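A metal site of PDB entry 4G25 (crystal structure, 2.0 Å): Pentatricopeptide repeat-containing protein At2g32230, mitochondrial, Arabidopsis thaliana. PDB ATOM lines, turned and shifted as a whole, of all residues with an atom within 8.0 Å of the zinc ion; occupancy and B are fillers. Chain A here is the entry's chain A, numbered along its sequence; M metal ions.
The zinc ion is bound by SG of Cys 276 (2.0 Å), NE2 of His 477 (2.1 Å), SG of Cys 494 (2.3 Å) and SG of Cys 273 (2.4 Å).
The zinc ion has four donor atoms within binding distance.
The backbone NH of Cys 273 sits at hydrogen-bond distance from the backbone carbonyl oxygen of Glu 278.
SD of Met 267 sits close to N of Cys 273 (3.6 Å).
The side-chain sulfur of Cys 276 lies close to the backbone NH of Glu 278 (3.5 Å).
The side-chain sulfur (SG) of Cys 273 lies close to the backbone NH (N) of Cys 275, at 3.3 Å.
N of Cys 494 lies within hydrogen-bond range of O of Lys 263, at 2.8 Å.
Four residues have an atom within 4 Å of the zinc ion: Cys 273, Cys 276, His 477 and Cys 494.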
ATOM      1  N   ASN A 261      15.546  -4.192  -1.258  1.00  0.00           N
ATOM      2  CA  ASN A 261      14.939  -2.879  -0.991  1.00  0.00           C
ATOM      3  C   ASN A 261      13.680  -3.062  -0.180  1.00  0.00           C
ATOM      4  O   ASN A 261      12.711  -3.668  -0.624  1.00  0.00           O
ATOM      5  CB  ASN A 261      14.648  -2.119  -2.292  1.00  0.00           C
ATOM      6  CG  ASN A 261      15.929  -1.685  -2.982  1.00  0.00           C
ATOM      7  OD1 ASN A 261      16.124  -1.928  -4.177  1.00  0.00           O
ATOM      8  ND2 ASN A 261      16.837  -1.070  -2.210  1.00  0.00           N
ATOM      9  N   LYS A 263      10.729  -1.312   2.011  1.00  0.00           N
ATOM     10  CA  LYS A 263      10.027  -0.048   2.275  1.00  0.00           C
ATOM     11  C   LYS A 263       8.690  -0.242   2.953  1.00  0.00           C
ATOM     12  O   LYS A 263       7.933  -1.143   2.578  1.00  0.00           O
ATOM     13  CB  LYS A 263       9.815   0.733   0.976  1.00  0.00           C
ATOM     14  CG  LYS A 263      11.021   1.548   0.499  1.00  0.00           C
ATOM     15  CD  LYS A 263      11.439   2.667   1.463  1.00  0.00           C
ATOM     16  CE  LYS A 263      10.268   3.553   1.938  1.00  0.00           C
ATOM     17  NZ  LYS A 263       9.553   4.240   0.815  1.00  0.00           N
ATOM     18  N   THR A 265       5.028   0.967   3.185  1.00  0.00           N
ATOM     19  CA  THR A 265       4.265   1.499   2.096  1.00  0.00           C
ATOM     20  C   THR A 265       2.747   1.237   2.336  1.00  0.00           C
ATOM     21  O   THR A 265       2.352   0.992   3.479  1.00  0.00           O
ATOM     22  CB  THR A 265       4.771   0.899   0.775  1.00  0.00           C
ATOM     23  OG1 THR A 265       4.261   1.642  -0.317  1.00  0.00           O
ATOM     24  CG2 THR A 265       4.339  -0.544   0.619  1.00  0.00           C
ATOM     25  N   GLU A 266       1.966   1.352   1.275  1.00  0.00           N
ATOM     26  CA  GLU A 266       0.510   1.220   1.275  1.00  0.00           C
ATOM     27  C   GLU A 266       0.090   0.690  -0.051  1.00  0.00           C
ATOM     28  O   GLU A 266       0.825   0.838  -1.027  1.00  0.00           O
ATOM     29  CB  GLU A 266      -0.175   2.570   1.471  1.00  0.00           C
ATOM     30  CG  GLU A 266      -0.263   3.020   2.916  1.00  0.00           C
ATOM     31  CD  GLU A 266      -0.763   4.484   3.064  1.00  0.00           C
ATOM     32  OE1 GLU A 266      -0.950   5.198   2.048  1.00  0.00           O
ATOM     33  OE2 GLU A 266      -0.963   4.906   4.222  1.00  0.00           O
ATOM     34  N   MET A 267      -1.080   0.038  -0.097  1.00  0.00           N
ATOM     35  CA  MET A 267      -1.671  -0.407  -1.323  1.00  0.00           C
ATOM     36  C   MET A 267      -2.718   0.631  -1.630  1.00  0.00           C
ATOM     37  O   MET A 267      -3.311   1.187  -0.728  1.00  0.00           O
ATOM     38  CB  MET A 267      -2.385  -1.752  -1.198  1.00  0.00           C
ATOM     39  CG  MET A 267      -1.491  -2.822  -0.644  1.00  0.00           C
ATOM     40  SD  MET A 267      -0.063  -3.250  -1.904  1.00  0.00           S
ATOM     41  CE  MET A 267       1.443  -2.797  -0.725  1.00  0.00           C
ATOM     42  N   VAL A 272      -2.636  -1.990  -5.623  1.00  0.00           N
ATOM     43  CA  VAL A 272      -1.344  -1.692  -6.287  1.00  0.00           C
ATOM     44  C   VAL A 272      -0.408  -1.087  -5.250  1.00  0.00           C
ATOM     45  O   VAL A 272      -0.736  -0.094  -4.631  1.00  0.00           O
ATOM     46  CB  VAL A 272      -1.487  -0.739  -7.496  1.00  0.00           C
ATOM     47  CG1 VAL A 272      -0.136  -0.480  -8.195  1.00  0.00           C
ATOM     48  CG2 VAL A 272      -2.470  -1.287  -8.499  1.00  0.00           C
ATOM     49  N   CYS A 273       0.724  -1.754  -5.028  1.00  0.00           N
ATOM     50  CA  CYS A 273       1.755  -1.280  -4.120  1.00  0.00           C
ATOM     51  C   CYS A 273       2.263   0.069  -4.607  1.00  0.00           C
ATOM     52  O   CYS A 273       2.672   0.206  -5.755  1.00  0.00           O
ATOM     53  CB  CYS A 273       2.975  -2.261  -4.050  1.00  0.00           C
ATOM     54  SG  CYS A 273       4.324  -1.619  -3.041  1.00  0.00           S
ATOM     55  N   LYS A 274       2.250   1.044  -3.728  1.00  0.00           N
ATOM     56  CA  LYS A 274       2.652   2.388  -4.124  1.00  0.00           C
ATOM     57  C   LYS A 274       4.164   2.522  -4.231  1.00  0.00           C
ATOM     58  O   LYS A 274       4.642   3.469  -4.820  1.00  0.00           O
ATOM     59  CB  LYS A 274       2.105   3.392  -3.150  1.00  0.00           C
ATOM     60  CG  LYS A 274       0.572   3.496  -3.254  1.00  0.00           C
ATOM     61  CD  LYS A 274       0.027   4.333  -2.117  1.00  0.00           C
ATOM     62  CE  LYS A 274      -1.489   4.516  -2.172  1.00  0.00           C
ATOM     63  NZ  LYS A 274      -1.850   5.212  -0.918  1.00  0.00           N
ATOM     64  N   CYS A 275       4.897   1.578  -3.634  1.00  0.00           N
ATOM     65  CA  CYS A 275       6.359   1.554  -3.693  1.00  0.00           C
ATOM     66  C   CYS A 275       6.770   0.981  -5.024  1.00  0.00           C
ATOM     67  O   CYS A 275       7.424   1.643  -5.805  1.00  0.00           O
ATOM     68  CB  CYS A 275       6.944   0.697  -2.562  1.00  0.00           C
ATOM     69  SG  CYS A 275       8.763   0.598  -2.564  1.00  0.00           S
ATOM     70  N   CYS A 276       6.344  -0.236  -5.323  1.00  0.00           N
ATOM     71  CA  CYS A 276       6.883  -0.965  -6.460  1.00  0.00           C
ATOM     72  C   CYS A 276       5.915  -1.127  -7.623  1.00  0.00           C
ATOM     73  O   CYS A 276       6.286  -1.632  -8.668  1.00  0.00           O
ATOM     74  CB  CYS A 276       7.394  -2.342  -5.981  1.00  0.00           C
ATOM     75  SG  CYS A 276       6.186  -3.679  -5.627  1.00  0.00           S
ATOM     76  N   LYS A 277       4.654  -0.734  -7.418  1.00  0.00           N
ATOM     77  CA  LYS A 277       3.589  -0.891  -8.413  1.00  0.00           C
ATOM     78  C   LYS A 277       3.145  -2.305  -8.718  1.00  0.00           C
ATOM     79  O   LYS A 277       2.460  -2.516  -9.677  1.00  0.00           O
ATOM     80  CB  LYS A 277       3.924  -0.171  -9.738  1.00  0.00           C
ATOM     81  CG  LYS A 277       4.421   1.243  -9.577  1.00  0.00           C
ATOM     82  CD  LYS A 277       3.584   2.098  -8.638  1.00  0.00           C
ATOM     83  CE  LYS A 277       4.021   3.558  -8.770  1.00  0.00           C
ATOM     84  NZ  LYS A 277       3.490   4.425  -7.684  1.00  0.00           N
ATOM     85  N   GLU A 278       3.521  -3.290  -7.924  1.00  0.00           N
ATOM     86  CA  GLU A 278       2.990  -4.615  -8.152  1.00  0.00           C
ATOM     87  C   GLU A 278       1.488  -4.602  -7.750  1.00  0.00           C
ATOM     88  O   GLU A 278       1.111  -3.961  -6.773  1.00  0.00           O
ATOM     89  CB  GLU A 278       3.774  -5.643  -7.352  1.00  0.00           C
ATOM     90  CG  GLU A 278       3.179  -7.059  -7.361  1.00  0.00           C
ATOM     91  CD  GLU A 278       4.167  -8.137  -7.729  1.00  0.00           C
ATOM     92  OE1 GLU A 278       5.398  -7.906  -7.635  1.00  0.00           O
ATOM     93  OE2 GLU A 278       3.714  -9.226  -8.137  1.00  0.00           O
ATOM     94  N   LYS A 279       0.672  -5.307  -8.510  1.00  0.00           N
ATOM     95  CA  LYS A 279      -0.759  -5.414  -8.254  1.00  0.00           C
ATOM     96  C   LYS A 279      -0.981  -6.681  -7.454  1.00  0.00           C
ATOM     97  O   LYS A 279      -0.760  -7.756  -7.976  1.00  0.00           O
ATOM     98  CB  LYS A 279      -1.523  -5.463  -9.572  1.00  0.00           C
ATOM     99  CG  LYS A 279      -2.915  -4.853  -9.504  1.00  0.00           C
ATOM    100  CD  LYS A 279      -3.978  -5.789  -8.949  1.00  0.00           C
ATOM    101  CE  LYS A 279      -4.153  -7.051  -9.801  1.00  0.00           C
ATOM    102  NZ  LYS A 279      -4.305  -6.767 -11.258  1.00  0.00           N
ATOM    103  N   LEU A 280      -1.409  -6.584  -6.202  1.00  0.00           N
ATOM    104  CA  LEU A 280      -1.660  -7.812  -5.444  1.00  0.00           C
ATOM    105  C   LEU A 280      -2.768  -8.698  -6.026  1.00  0.00           C
ATOM    106  O   LEU A 280      -3.604  -8.245  -6.763  1.00  0.00           O
ATOM    107  CB  LEU A 280      -1.950  -7.494  -3.985  1.00  0.00           C
ATOM    108  CG  LEU A 280      -0.729  -6.868  -3.285  1.00  0.00           C
ATOM    109  CD1 LEU A 280      -0.983  -6.703  -1.801  1.00  0.00           C
ATOM    110  CD2 LEU A 280       0.548  -7.655  -3.503  1.00  0.00           C
ATOM    111  N   THR A 475       9.208 -11.309  -4.918  1.00  0.00           N
ATOM    112  CA  THR A 475       8.888 -10.061  -4.179  1.00  0.00           C
ATOM    113  C   THR A 475       7.842 -10.327  -3.087  1.00  0.00           C
ATOM    114  O   THR A 475       6.864 -11.039  -3.306  1.00  0.00           O
ATOM    115  CB  THR A 475       8.381  -8.977  -5.149  1.00  0.00           C
ATOM    116  OG1 THR A 475       9.415  -8.731  -6.107  1.00  0.00           O
ATOM    117  CG2 THR A 475       8.057  -7.671  -4.421  1.00  0.00           C
ATOM    118  N   TRP A 476       8.065  -9.780  -1.886  1.00  0.00           N
ATOM    119  CA  TRP A 476       7.118  -9.949  -0.773  1.00  0.00           C
ATOM    120  C   TRP A 476       6.356  -8.700  -0.471  1.00  0.00           C
ATOM    121  O   TRP A 476       6.940  -7.632  -0.463  1.00  0.00           O
ATOM    122  CB  TRP A 476       7.811 -10.407   0.480  1.00  0.00           C
ATOM    123  CG  TRP A 476       8.338 -11.789   0.362  1.00  0.00           C
ATOM    124  CD1 TRP A 476       9.482 -12.205  -0.269  1.00  0.00           C
ATOM    125  CD2 TRP A 476       7.757 -12.972   0.937  1.00  0.00           C
ATOM    126  NE1 TRP A 476       9.652 -13.558  -0.133  1.00  0.00           N
ATOM    127  CE2 TRP A 476       8.647 -14.079   0.576  1.00  0.00           C
ATOM    128  CE3 TRP A 476       6.635 -13.239   1.687  1.00  0.00           C
ATOM    129  CZ2 TRP A 476       8.390 -15.367   0.941  1.00  0.00           C
ATOM    130  CZ3 TRP A 476       6.387 -14.537   2.081  1.00  0.00           C
ATOM    131  CH2 TRP A 476       7.256 -15.586   1.720  1.00  0.00           C
ATOM    132  N   HIS A 477       5.065  -8.861  -0.144  1.00  0.00           N
ATOM    133  CA  HIS A 477       4.256  -7.783   0.422  1.00  0.00           C
ATOM    134  C   HIS A 477       3.600  -8.301   1.693  1.00  0.00           C
ATOM    135  O   HIS A 477       2.902  -9.328   1.682  1.00  0.00           O
ATOM    136  CB  HIS A 477       3.253  -7.305  -0.629  1.00  0.00           C
ATOM    137  CG  HIS A 477       3.893  -6.627  -1.804  1.00  0.00           C
ATOM    138  ND1 HIS A 477       4.138  -7.270  -2.935  1.00  0.00           N
ATOM    139  CD2 HIS A 477       4.395  -5.319  -1.986  1.00  0.00           C
ATOM    140  CE1 HIS A 477       4.740  -6.432  -3.812  1.00  0.00           C
ATOM    141  NE2 HIS A 477       4.882  -5.255  -3.225  1.00  0.00           N
ATOM    142  N   VAL A 478       3.862  -7.631   2.787  1.00  0.00           N
ATOM    143  CA  VAL A 478       3.442  -8.052   4.109  1.00  0.00           C
ATOM    144  C   VAL A 478       2.529  -6.977   4.752  1.00  0.00           C
ATOM    145  O   VAL A 478       2.994  -5.885   5.046  1.00  0.00           O
ATOM    146  CB  VAL A 478       4.658  -8.259   5.002  1.00  0.00           C
ATOM    147  CG1 VAL A 478       4.233  -8.615   6.409  1.00  0.00           C
ATOM    148  CG2 VAL A 478       5.619  -9.311   4.386  1.00  0.00           C
ATOM    149  N   TRP A 492       1.953  -1.590   5.009  1.00  0.00           N
ATOM    150  CA  TRP A 492       2.534  -2.780   4.405  1.00  0.00           C
ATOM    151  C   TRP A 492       4.039  -2.668   4.307  1.00  0.00           C
ATOM    152  O   TRP A 492       4.618  -1.555   4.272  1.00  0.00           O
ATOM    153  CB  TRP A 492       2.026  -2.970   3.004  1.00  0.00           C
ATOM    154  CG  TRP A 492       0.575  -3.375   2.853  1.00  0.00           C
ATOM    155  CD1 TRP A 492      -0.590  -2.591   3.052  1.00  0.00           C
ATOM    156  CD2 TRP A 492       0.090  -4.675   2.389  1.00  0.00           C
ATOM    157  NE1 TRP A 492      -1.720  -3.304   2.736  1.00  0.00           N
ATOM    158  CE2 TRP A 492      -1.384  -4.561   2.312  1.00  0.00           C
ATOM    159  CE3 TRP A 492       0.694  -5.844   1.975  1.00  0.00           C
ATOM    160  CZ2 TRP A 492      -2.158  -5.632   1.914  1.00  0.00           C
ATOM    161  CZ3 TRP A 492      -0.105  -6.923   1.594  1.00  0.00           C
ATOM    162  CH2 TRP A 492      -1.502  -6.797   1.517  1.00  0.00           C
ATOM    163  N   LEU A 493       4.685  -3.822   4.174  1.00  0.00           N
ATOM    164  CA  LEU A 493       6.070  -3.900   3.857  1.00  0.00           C
ATOM    165  C   LEU A 493       6.190  -4.332   2.435  1.00  0.00           C
ATOM    166  O   LEU A 493       5.519  -5.286   2.012  1.00  0.00           O
ATOM    167  CB  LEU A 493       6.771  -4.880   4.807  1.00  0.00           C
ATOM    168  CG  LEU A 493       8.278  -4.674   5.014  1.00  0.00           C
ATOM    169  CD1 LEU A 493       8.580  -3.311   5.629  1.00  0.00           C
ATOM    170  CD2 LEU A 493       8.848  -5.775   5.903  1.00  0.00           C
ATOM    171  N   CYS A 494       7.036  -3.639   1.670  1.00  0.00           N
ATOM    172  CA  CYS A 494       7.395  -4.042   0.307  1.00  0.00           C
ATOM    173  C   CYS A 494       8.884  -4.487   0.333  1.00  0.00           C
ATOM    174  O   CYS A 494       9.730  -3.651   0.665  1.00  0.00           O
ATOM    175  CB  CYS A 494       7.293  -2.884  -0.655  1.00  0.00           C
ATOM    176  SG  CYS A 494       7.759  -3.248  -2.372  1.00  0.00           S
ATOM    177  N   ALA A 495       9.186  -5.749   0.012  1.00  0.00           N
ATOM    178  CA  ALA A 495      10.572  -6.272   0.027  1.00  0.00           C
ATOM    179  C   ALA A 495      10.863  -6.807  -1.330  1.00  0.00           C
ATOM    180  O   ALA A 495      10.306  -7.808  -1.766  1.00  0.00           O
ATOM    181  CB  ALA A 495      10.731  -7.352   1.088  1.00  0.00           C
ATOM    182  N   LYS A 496      11.690  -6.065  -2.059  1.00  0.00           N
ATOM    183  CA  LYS A 496      11.981  -6.379  -3.450  1.00  0.00           C
ATOM    184  C   LYS A 496      13.518  -6.359  -3.679  1.00  0.00           C
ATOM    185  O   LYS A 496      14.163  -5.420  -3.256  1.00  0.00           O
ATOM    186  CB  LYS A 496      11.351  -5.306  -4.333  1.00  0.00           C
ATOM    187  CG  LYS A 496      11.405  -5.603  -5.804  1.00  0.00           C
ATOM    188  CD  LYS A 496      10.597  -4.573  -6.585  1.00  0.00           C
ATOM    189  CE  LYS A 496      10.474  -5.012  -8.027  1.00  0.00           C
ATOM    190  NZ  LYS A 496       9.699  -6.287  -8.116  1.00  0.00           N
HETATM  191 ZN    ZN M   1       5.818  -3.430  -3.676  1.00  0.00          ZN
